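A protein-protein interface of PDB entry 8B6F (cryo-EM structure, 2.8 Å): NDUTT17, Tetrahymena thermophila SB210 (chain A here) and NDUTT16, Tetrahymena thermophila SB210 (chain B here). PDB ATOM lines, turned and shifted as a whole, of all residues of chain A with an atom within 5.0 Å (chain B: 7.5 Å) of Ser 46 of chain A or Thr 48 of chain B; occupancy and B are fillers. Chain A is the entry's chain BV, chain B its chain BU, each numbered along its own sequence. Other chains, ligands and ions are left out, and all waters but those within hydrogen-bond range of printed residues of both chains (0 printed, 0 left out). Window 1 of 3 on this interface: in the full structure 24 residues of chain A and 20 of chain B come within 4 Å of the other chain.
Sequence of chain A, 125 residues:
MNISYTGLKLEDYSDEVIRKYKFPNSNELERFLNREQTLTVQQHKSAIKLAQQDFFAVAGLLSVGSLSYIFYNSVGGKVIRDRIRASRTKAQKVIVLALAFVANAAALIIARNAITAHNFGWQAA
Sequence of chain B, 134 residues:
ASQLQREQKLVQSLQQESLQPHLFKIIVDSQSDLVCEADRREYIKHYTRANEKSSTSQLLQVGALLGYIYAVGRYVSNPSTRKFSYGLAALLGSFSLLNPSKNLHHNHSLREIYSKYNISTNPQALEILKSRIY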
ATOM      1  N   GLN A  42       9.989  24.513  30.410  1.00  0.00           N
ATOM      2  CA  GLN A  42       9.684  25.800  29.798  1.00  0.00           C
ATOM      3  C   GLN A  42       8.194  26.102  29.871  1.00  0.00           C
ATOM      4  O   GLN A  42       7.800  27.258  30.057  1.00  0.00           O
ATOM      5  CB  GLN A  42      10.161  25.824  28.350  1.00  0.00           C
ATOM      6  CG  GLN A  42      10.243  27.219  27.774  1.00  0.00           C
ATOM      7  CD  GLN A  42      11.322  28.055  28.435  1.00  0.00           C
ATOM      8  OE1 GLN A  42      12.145  27.541  29.190  1.00  0.00           O
ATOM      9  NE2 GLN A  42      11.322  29.352  28.151  1.00  0.00           N
ATOM     10  N   GLN A  43       7.348  25.083  29.715  1.00  0.00           N
ATOM     11  CA  GLN A  43       5.918  25.289  29.916  1.00  0.00           C
ATOM     12  C   GLN A  43       5.629  25.721  31.347  1.00  0.00           C
ATOM     13  O   GLN A  43       4.810  26.616  31.580  1.00  0.00           O
ATOM     14  CB  GLN A  43       5.148  24.015  29.572  1.00  0.00           C
ATOM     15  CG  GLN A  43       4.910  23.825  28.085  1.00  0.00           C
ATOM     16  CD  GLN A  43       4.278  22.488  27.762  1.00  0.00           C
ATOM     17  OE1 GLN A  43       4.427  21.522  28.508  1.00  0.00           O
ATOM     18  NE2 GLN A  43       3.562  22.427  26.646  1.00  0.00           N
ATOM     19  N   HIS A  44       6.284  25.088  32.323  1.00  0.00           N
ATOM     20  CA  HIS A  44       6.109  25.501  33.711  1.00  0.00           C
ATOM     21  C   HIS A  44       6.548  26.946  33.907  1.00  0.00           C
ATOM     22  O   HIS A  44       5.863  27.725  34.579  1.00  0.00           O
ATOM     23  CB  HIS A  44       6.899  24.579  34.639  1.00  0.00           C
ATOM     24  CG  HIS A  44       6.334  23.197  34.741  1.00  0.00           C
ATOM     25  ND1 HIS A  44       5.343  22.865  35.639  1.00  0.00           N
ATOM     26  CD2 HIS A  44       6.620  22.064  34.060  1.00  0.00           C
ATOM     27  CE1 HIS A  44       5.043  21.585  35.505  1.00  0.00           C
ATOM     28  NE2 HIS A  44       5.803  21.076  34.554  1.00  0.00           N
ATOM     29  N   LYS A  45       7.687  27.322  33.321  1.00  0.00           N
ATOM     30  CA  LYS A  45       8.183  28.686  33.474  1.00  0.00           C
ATOM     31  C   LYS A  45       7.234  29.691  32.836  1.00  0.00           C
ATOM     32  O   LYS A  45       6.977  30.760  33.402  1.00  0.00           O
ATOM     33  CB  LYS A  45       9.581  28.808  32.866  1.00  0.00           C
ATOM     34  CG  LYS A  45      10.648  27.996  33.589  1.00  0.00           C
ATOM     35  CD  LYS A  45      11.029  28.601  34.936  1.00  0.00           C
ATOM     36  CE  LYS A  45      11.844  29.875  34.773  1.00  0.00           C
ATOM     37  NZ  LYS A  45      12.351  30.379  36.081  1.00  0.00           N
ATOM     38  N   SER A  46       6.705  29.369  31.657  1.00  0.00           N
ATOM     39  CA  SER A  46       5.751  30.263  31.010  1.00  0.00           C
ATOM     40  C   SER A  46       4.486  30.413  31.842  1.00  0.00           C
ATOM     41  O   SER A  46       3.955  31.521  31.986  1.00  0.00           O
ATOM     42  CB  SER A  46       5.413  29.744  29.614  1.00  0.00           C
ATOM     43  OG  SER A  46       4.469  30.587  28.977  1.00  0.00           O
ATOM     44  N   ALA A  47       3.983  29.309  32.394  1.00  0.00           N
ATOM     45  CA  ALA A  47       2.800  29.384  33.245  1.00  0.00           C
ATOM     46  C   ALA A  47       3.060  30.251  34.469  1.00  0.00           C
ATOM     47  O   ALA A  47       2.213  31.061  34.858  1.00  0.00           O
ATOM     48  CB  ALA A  47       2.368  27.979  33.662  1.00  0.00           C
ATOM     49  N   ILE A  48       4.231  30.093  35.092  1.00  0.00           N
ATOM     50  CA  ILE A  48       4.569  30.895  36.264  1.00  0.00           C
ATOM     51  C   ILE A  48       4.658  32.369  35.893  1.00  0.00           C
ATOM     52  O   ILE A  48       4.156  33.236  36.617  1.00  0.00           O
ATOM     53  CB  ILE A  48       5.881  30.393  36.893  1.00  0.00           C
ATOM     54  CG1 ILE A  48       5.674  29.014  37.510  1.00  0.00           C
ATOM     55  CG2 ILE A  48       6.375  31.358  37.963  1.00  0.00           C
ATOM     56  CD1 ILE A  48       6.958  28.306  37.849  1.00  0.00           C
ATOM     57  N   LYS A  49       5.285  32.676  34.757  1.00  0.00           N
ATOM     58  CA  LYS A  49       5.400  34.069  34.339  1.00  0.00           C
ATOM     59  C   LYS A  49       4.023  34.683  34.129  1.00  0.00           C
ATOM     60  O   LYS A  49       3.757  35.806  34.571  1.00  0.00           O
ATOM     61  CB  LYS A  49       6.234  34.164  33.061  1.00  0.00           C
ATOM     62  CG  LYS A  49       6.576  35.591  32.658  1.00  0.00           C
ATOM     63  CD  LYS A  49       7.226  35.655  31.285  1.00  0.00           C
ATOM     64  CE  LYS A  49       6.212  35.411  30.179  1.00  0.00           C
ATOM     65  NZ  LYS A  49       6.805  35.609  28.829  1.00  0.00           N
ATOM     66  N   LEU A  50       3.132  33.959  33.454  1.00  0.00           N
ATOM     67  CA  LEU A  50       1.780  34.463  33.249  1.00  0.00           C
ATOM     68  C   LEU A  50       1.059  34.642  34.577  1.00  0.00           C
ATOM     69  O   LEU A  50       0.322  35.617  34.767  1.00  0.00           O
ATOM     70  CB  LEU A  50       0.999  33.516  32.340  1.00  0.00           C
ATOM     71  CG  LEU A  50       1.439  33.481  30.875  1.00  0.00           C
ATOM     72  CD1 LEU A  50       0.725  32.362  30.142  1.00  0.00           C
ATOM     73  CD2 LEU A  50       1.179  34.815  30.195  1.00  0.00           C
ATOM     74  N   ALA A  51       1.251  33.706  35.509  1.00  0.00           N
ATOM     75  CA  ALA A  51       0.600  33.813  36.810  1.00  0.00           C
ATOM     76  C   ALA A  51       1.068  35.055  37.556  1.00  0.00           C
ATOM     77  O   ALA A  51       0.257  35.807  38.106  1.00  0.00           O
ATOM     78  CB  ALA A  51       0.877  32.557  37.635  1.00  0.00           C
ATOM     79  N   LYS B  25       3.116  20.855  15.717  1.00  0.00           N
ATOM     80  CA  LYS B  25       2.818  20.825  17.144  1.00  0.00           C
ATOM     81  C   LYS B  25       2.026  19.575  17.503  1.00  0.00           C
ATOM     82  O   LYS B  25       2.253  18.969  18.556  1.00  0.00           O
ATOM     83  CB  LYS B  25       2.049  22.082  17.549  1.00  0.00           C
ATOM     84  CG  LYS B  25       1.758  22.185  19.043  1.00  0.00           C
ATOM     85  CD  LYS B  25       3.047  22.234  19.856  1.00  0.00           C
ATOM     86  CE  LYS B  25       2.768  22.398  21.337  1.00  0.00           C
ATOM     87  NZ  LYS B  25       2.044  21.227  21.898  1.00  0.00           N
ATOM     88  N   ARG B  41      11.682  19.757  22.311  1.00  0.00           N
ATOM     89  CA  ARG B  41      11.685  20.712  23.415  1.00  0.00           C
ATOM     90  C   ARG B  41      11.775  22.144  22.905  1.00  0.00           C
ATOM     91  O   ARG B  41      11.067  23.031  23.397  1.00  0.00           O
ATOM     92  CB  ARG B  41      12.838  20.404  24.369  1.00  0.00           C
ATOM     93  CG  ARG B  41      12.994  21.415  25.494  1.00  0.00           C
ATOM     94  CD  ARG B  41      14.019  20.957  26.518  1.00  0.00           C
ATOM     95  NE  ARG B  41      15.315  20.670  25.911  1.00  0.00           N
ATOM     96  CZ  ARG B  41      15.725  19.465  25.536  1.00  0.00           C
ATOM     97  NH1 ARG B  41      14.964  18.393  25.690  1.00  0.00           N
ATOM     98  NH2 ARG B  41      16.930  19.330  24.988  1.00  0.00           N
ATOM     99  N   GLU B  42      12.642  22.391  21.922  1.00  0.00           N
ATOM    100  CA  GLU B  42      12.767  23.733  21.361  1.00  0.00           C
ATOM    101  C   GLU B  42      11.460  24.188  20.729  1.00  0.00           C
ATOM    102  O   GLU B  42      11.042  25.337  20.908  1.00  0.00           O
ATOM    103  CB  GLU B  42      13.896  23.768  20.331  1.00  0.00           C
ATOM    104  CG  GLU B  42      15.284  23.599  20.924  1.00  0.00           C
ATOM    105  CD  GLU B  42      15.698  24.783  21.777  1.00  0.00           C
ATOM    106  OE1 GLU B  42      14.977  25.801  21.773  1.00  0.00           O
ATOM    107  OE2 GLU B  42      16.747  24.695  22.450  1.00  0.00           O
ATOM    108  N   TYR B  43      10.802  23.301  19.983  1.00  0.00           N
ATOM    109  CA  TYR B  43       9.539  23.665  19.352  1.00  0.00           C
ATOM    110  C   TYR B  43       8.465  23.952  20.393  1.00  0.00           C
ATOM    111  O   TYR B  43       7.676  24.890  20.238  1.00  0.00           O
ATOM    112  CB  TYR B  43       9.084  22.555  18.407  1.00  0.00           C
ATOM    113  CG  TYR B  43       7.936  22.966  17.521  1.00  0.00           C
ATOM    114  CD1 TYR B  43       8.164  23.560  16.287  1.00  0.00           C
ATOM    115  CD2 TYR B  43       6.623  22.770  17.922  1.00  0.00           C
ATOM    116  CE1 TYR B  43       7.117  23.942  15.477  1.00  0.00           C
ATOM    117  CE2 TYR B  43       5.570  23.148  17.119  1.00  0.00           C
ATOM    118  CZ  TYR B  43       5.822  23.732  15.898  1.00  0.00           C
ATOM    119  OH  TYR B  43       4.769  24.108  15.098  1.00  0.00           O
ATOM    120  N   ILE B  44       8.413  23.153  21.459  1.00  0.00           N
ATOM    121  CA  ILE B  44       7.443  23.406  22.521  1.00  0.00           C
ATOM    122  C   ILE B  44       7.691  24.776  23.139  1.00  0.00           C
ATOM    123  O   ILE B  44       6.757  25.552  23.369  1.00  0.00           O
ATOM    124  CB  ILE B  44       7.501  22.287  23.579  1.00  0.00           C
ATOM    125  CG1 ILE B  44       6.978  20.976  22.989  1.00  0.00           C
ATOM    126  CG2 ILE B  44       6.690  22.666  24.816  1.00  0.00           C
ATOM    127  CD1 ILE B  44       7.190  19.765  23.879  1.00  0.00           C
ATOM    128  N   LYS B  45       8.956  25.092  23.426  1.00  0.00           N
ATOM    129  CA  LYS B  45       9.273  26.392  24.006  1.00  0.00           C
ATOM    130  C   LYS B  45       8.800  27.522  23.104  1.00  0.00           C
ATOM    131  O   LYS B  45       8.086  28.430  23.546  1.00  0.00           O
ATOM    132  CB  LYS B  45      10.779  26.496  24.249  1.00  0.00           C
ATOM    133  CG  LYS B  45      11.275  27.923  24.446  1.00  0.00           C
ATOM    134  CD  LYS B  45      12.676  27.954  25.032  1.00  0.00           C
ATOM    135  CE  LYS B  45      13.723  27.502  24.028  1.00  0.00           C
ATOM    136  NZ  LYS B  45      13.833  28.435  22.872  1.00  0.00           N
ATOM    137  N   HIS B  46       9.190  27.484  21.829  1.00  0.00           N
ATOM    138  CA  HIS B  46       8.844  28.570  20.920  1.00  0.00           C
ATOM    139  C   HIS B  46       7.338  28.663  20.723  1.00  0.00           C
ATOM    140  O   HIS B  46       6.771  29.761  20.703  1.00  0.00           O
ATOM    141  CB  HIS B  46       9.554  28.378  19.580  1.00  0.00           C
ATOM    142  CG  HIS B  46      11.029  28.625  19.640  1.00  0.00           C
ATOM    143  ND1 HIS B  46      11.564  29.856  19.956  1.00  0.00           N
ATOM    144  CD2 HIS B  46      12.081  27.803  19.422  1.00  0.00           C
ATOM    145  CE1 HIS B  46      12.883  29.778  19.932  1.00  0.00           C
ATOM    146  NE2 HIS B  46      13.222  28.544  19.610  1.00  0.00           N
ATOM    147  N   TYR B  47       6.670  27.517  20.573  1.00  0.00           N
ATOM    148  CA  TYR B  47       5.228  27.523  20.354  1.00  0.00           C
ATOM    149  C   TYR B  47       4.490  28.084  21.560  1.00  0.00           C
ATOM    150  O   TYR B  47       3.562  28.887  21.412  1.00  0.00           O
ATOM    151  CB  TYR B  47       4.745  26.106  20.039  1.00  0.00           C
ATOM    152  CG  TYR B  47       3.360  26.039  19.439  1.00  0.00           C
ATOM    153  CD1 TYR B  47       3.171  26.133  18.064  1.00  0.00           C
ATOM    154  CD2 TYR B  47       2.241  25.868  20.243  1.00  0.00           C
ATOM    155  CE1 TYR B  47       1.906  26.067  17.510  1.00  0.00           C
ATOM    156  CE2 TYR B  47       0.972  25.801  19.698  1.00  0.00           C
ATOM    157  CZ  TYR B  47       0.811  25.900  18.332  1.00  0.00           C
ATOM    158  OH  TYR B  47      -0.450  25.835  17.786  1.00  0.00           O
ATOM    159  N   THR B  48       4.885  27.675  22.767  1.00  0.00           N
ATOM    160  CA  THR B  48       4.247  28.205  23.966  1.00  0.00           C
ATOM    161  C   THR B  48       4.473  29.707  24.088  1.00  0.00           C
ATOM    162  O   THR B  48       3.544  30.459  24.404  1.00  0.00           O
ATOM    163  CB  THR B  48       4.781  27.485  25.205  1.00  0.00           C
ATOM    164  OG1 THR B  48       4.589  26.073  25.062  1.00  0.00           O
ATOM    165  CG2 THR B  48       4.062  27.964  26.460  1.00  0.00           C
ATOM    166  N   ARG B  49       5.701  30.163  23.835  1.00  0.00           N
ATOM    167  CA  ARG B  49       5.995  31.588  23.934  1.00  0.00           C
ATOM    168  C   ARG B  49       5.182  32.391  22.927  1.00  0.00           C
ATOM    169  O   ARG B  49       4.686  33.478  23.244  1.00  0.00           O
ATOM    170  CB  ARG B  49       7.491  31.825  23.732  1.00  0.00           C
ATOM    171  CG  ARG B  49       7.917  33.269  23.938  1.00  0.00           C
ATOM    172  CD  ARG B  49       9.423  33.433  23.785  1.00  0.00           C
ATOM    173  NE  ARG B  49       9.844  34.811  24.012  1.00  0.00           N
ATOM    174  CZ  ARG B  49      11.097  35.235  23.940  1.00  0.00           C
ATOM    175  NH1 ARG B  49      12.090  34.413  23.642  1.00  0.00           N
ATOM    176  NH2 ARG B  49      11.363  36.517  24.172  1.00  0.00           N
ATOM    177  N   ALA B  50       5.039  31.875  21.706  1.00  0.00           N
ATOM    178  CA  ALA B  50       4.307  32.603  20.677  1.00  0.00           C
ATOM    179  C   ALA B  50       2.810  32.627  20.963  1.00  0.00           C
ATOM    180  O   ALA B  50       2.150  33.652  20.759  1.00  0.00           O
ATOM    181  CB  ALA B  50       4.576  31.984  19.307  1.00  0.00           C
ATOM    182  N   ASN B  51       2.254  31.508  21.430  1.00  0.00           N
ATOM    183  CA  ASN B  51       0.810  31.397  21.592  1.00  0.00           C
ATOM    184  C   ASN B  51       0.300  31.980  22.901  1.00  0.00           C
ATOM    185  O   ASN B  51      -0.885  32.323  22.985  1.00  0.00           O
ATOM    186  CB  ASN B  51       0.387  29.930  21.499  1.00  0.00           C
ATOM    187  CG  ASN B  51       0.476  29.389  20.088  1.00  0.00           C
ATOM    188  OD1 ASN B  51      -0.525  29.313  19.377  1.00  0.00           O
ATOM    189  ND2 ASN B  51       1.680  29.016  19.672  1.00  0.00           N
ATOM    190  N   GLU B  52       1.146  32.102  23.920  1.00  0.00           N
ATOM    191  CA  GLU B  52       0.676  32.559  25.221  1.00  0.00           C
ATOM    192  C   GLU B  52       0.032  33.936  25.108  1.00  0.00           C
ATOM    193  O   GLU B  52       0.571  34.836  24.458  1.00  0.00           O
ATOM    194  CB  GLU B  52       1.830  32.595  26.224  1.00  0.00           C
ATOM    195  CG  GLU B  52       2.845  33.700  25.987  1.00  0.00           C
ATOM    196  CD  GLU B  52       4.017  33.626  26.946  1.00  0.00           C
ATOM    197  OE1 GLU B  52       4.152  32.598  27.642  1.00  0.00           O
ATOM    198  OE2 GLU B  52       4.801  34.595  27.007  1.00  0.00           O
ATOM    199  N   LYS B  53      -1.126  34.092  25.742  1.00  0.00           N
ATOM    200  CA  LYS B  53      -1.830  35.367  25.800  1.00  0.00           C
ATOM    201  C   LYS B  53      -1.563  36.003  27.157  1.00  0.00           C
ATOM    202  O   LYS B  53      -1.815  35.385  28.196  1.00  0.00           O
ATOM    203  CB  LYS B  53      -3.331  35.180  25.583  1.00  0.00           C
ATOM    204  CG  LYS B  53      -3.699  34.668  24.200  1.00  0.00           C
ATOM    205  CD  LYS B  53      -5.206  34.545  24.043  1.00  0.00           C
ATOM    206  CE  LYS B  53      -5.583  34.049  22.657  1.00  0.00           C
ATOM    207  NZ  LYS B  53      -5.133  34.980  21.585  1.00  0.00           N
ATOM    208  N   LEU B 110      10.131  28.413  14.652  1.00  0.00           N
ATOM    209  CA  LEU B 110       9.294  27.242  14.420  1.00  0.00           C
ATOM    210  C   LEU B 110       9.506  26.684  13.019  1.00  0.00           C
ATOM    211  O   LEU B 110       9.640  25.468  12.840  1.00  0.00           O
ATOM    212  CB  LEU B 110       7.824  27.599  14.635  1.00  0.00           C
ATOM    213  CG  LEU B 110       7.477  28.188  16.003  1.00  0.00           C
ATOM    214  CD1 LEU B 110       6.037  28.659  16.025  1.00  0.00           C
ATOM    215  CD2 LEU B 110       7.727  27.176  17.109  1.00  0.00           C
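OG of Ser 46 of chain A is in hydrogen-bond range of OE1 of Glu 52 of chain B (2.4 Å). The side-chain amino group (NZ) of Lys 49 of chain A is in salt-bridge range of the side-chain carboxylate (OE2) of Glu 52 of chain B, at 2.9 Å.
OE1 of Glu 42 of chain B is in salt-bridge range of NZ of Lys 45 of chain B. The side-chain hydroxyl of Thr 48 of chain B is in hydrogen-bond range of the backbone carbonyl oxygen of Ile 44 of chain B (2.8 Å). The side-chain amino group of Lys 45 of chain B sits at hydrogen-bond distance from a ring nitrogen (NE2) of His 46 of chain B (3.3 Å).
Among the printed residues, merely in contact across the chains: Gln 42 of chain A with Lys 45 of chain B (3.6 Å), Gln 43 of chain A with Ile 44 of chain B (3.6 Å), Gln 43 of chain A with Thr 48 of chain B (3.8 Å), Ser 46 of chain A with Thr 48 of chain B (3.7 Å) and Leu 50 of chain A with Lys 53 of chain B (3.6 Å).
Ser 46 of chain A touches just these residues of chain B: Thr 48 and Glu 52. Of chain A, only Gln 43 and Ser 46 come within 4 Å of Thr 48 of chain B. Printed residues of chain B within 4 Å of Gln 42 of chain A: Lys 45 (3.6 Å). Of the printed residues of chain B, Leu 50 of chain A touches Lys 53. Of the printed residues of chain A, Lys 53 of chain B touches Leu 50. Printed residues of chain A within 4 Å of Lys 45 of chain B: Gln 42. Ala 50 of chain B touches none of the printed residues of chain A. The nearest printed residue of chain A that does not touch Thr 48 of chain B is Gln 42 of chain A (5.2 Å). The nearest printed residue of chain B that does not touch Leu 50 of chain A is Glu 52 of chain B (4.1 Å).
Of the 15 printed residues of chain B, 5 touch a printed residue of chain A. Hydrophobic or aromatic side chains of chain B that line the printed part of chain A: Ile 44. Printed residues of chain A that touch a printed residue of chain B: Gln 42, Gln 43, Ser 46, Lys 49 and Leu 50. Among the printed residues, 7 pairs touch across the chains.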
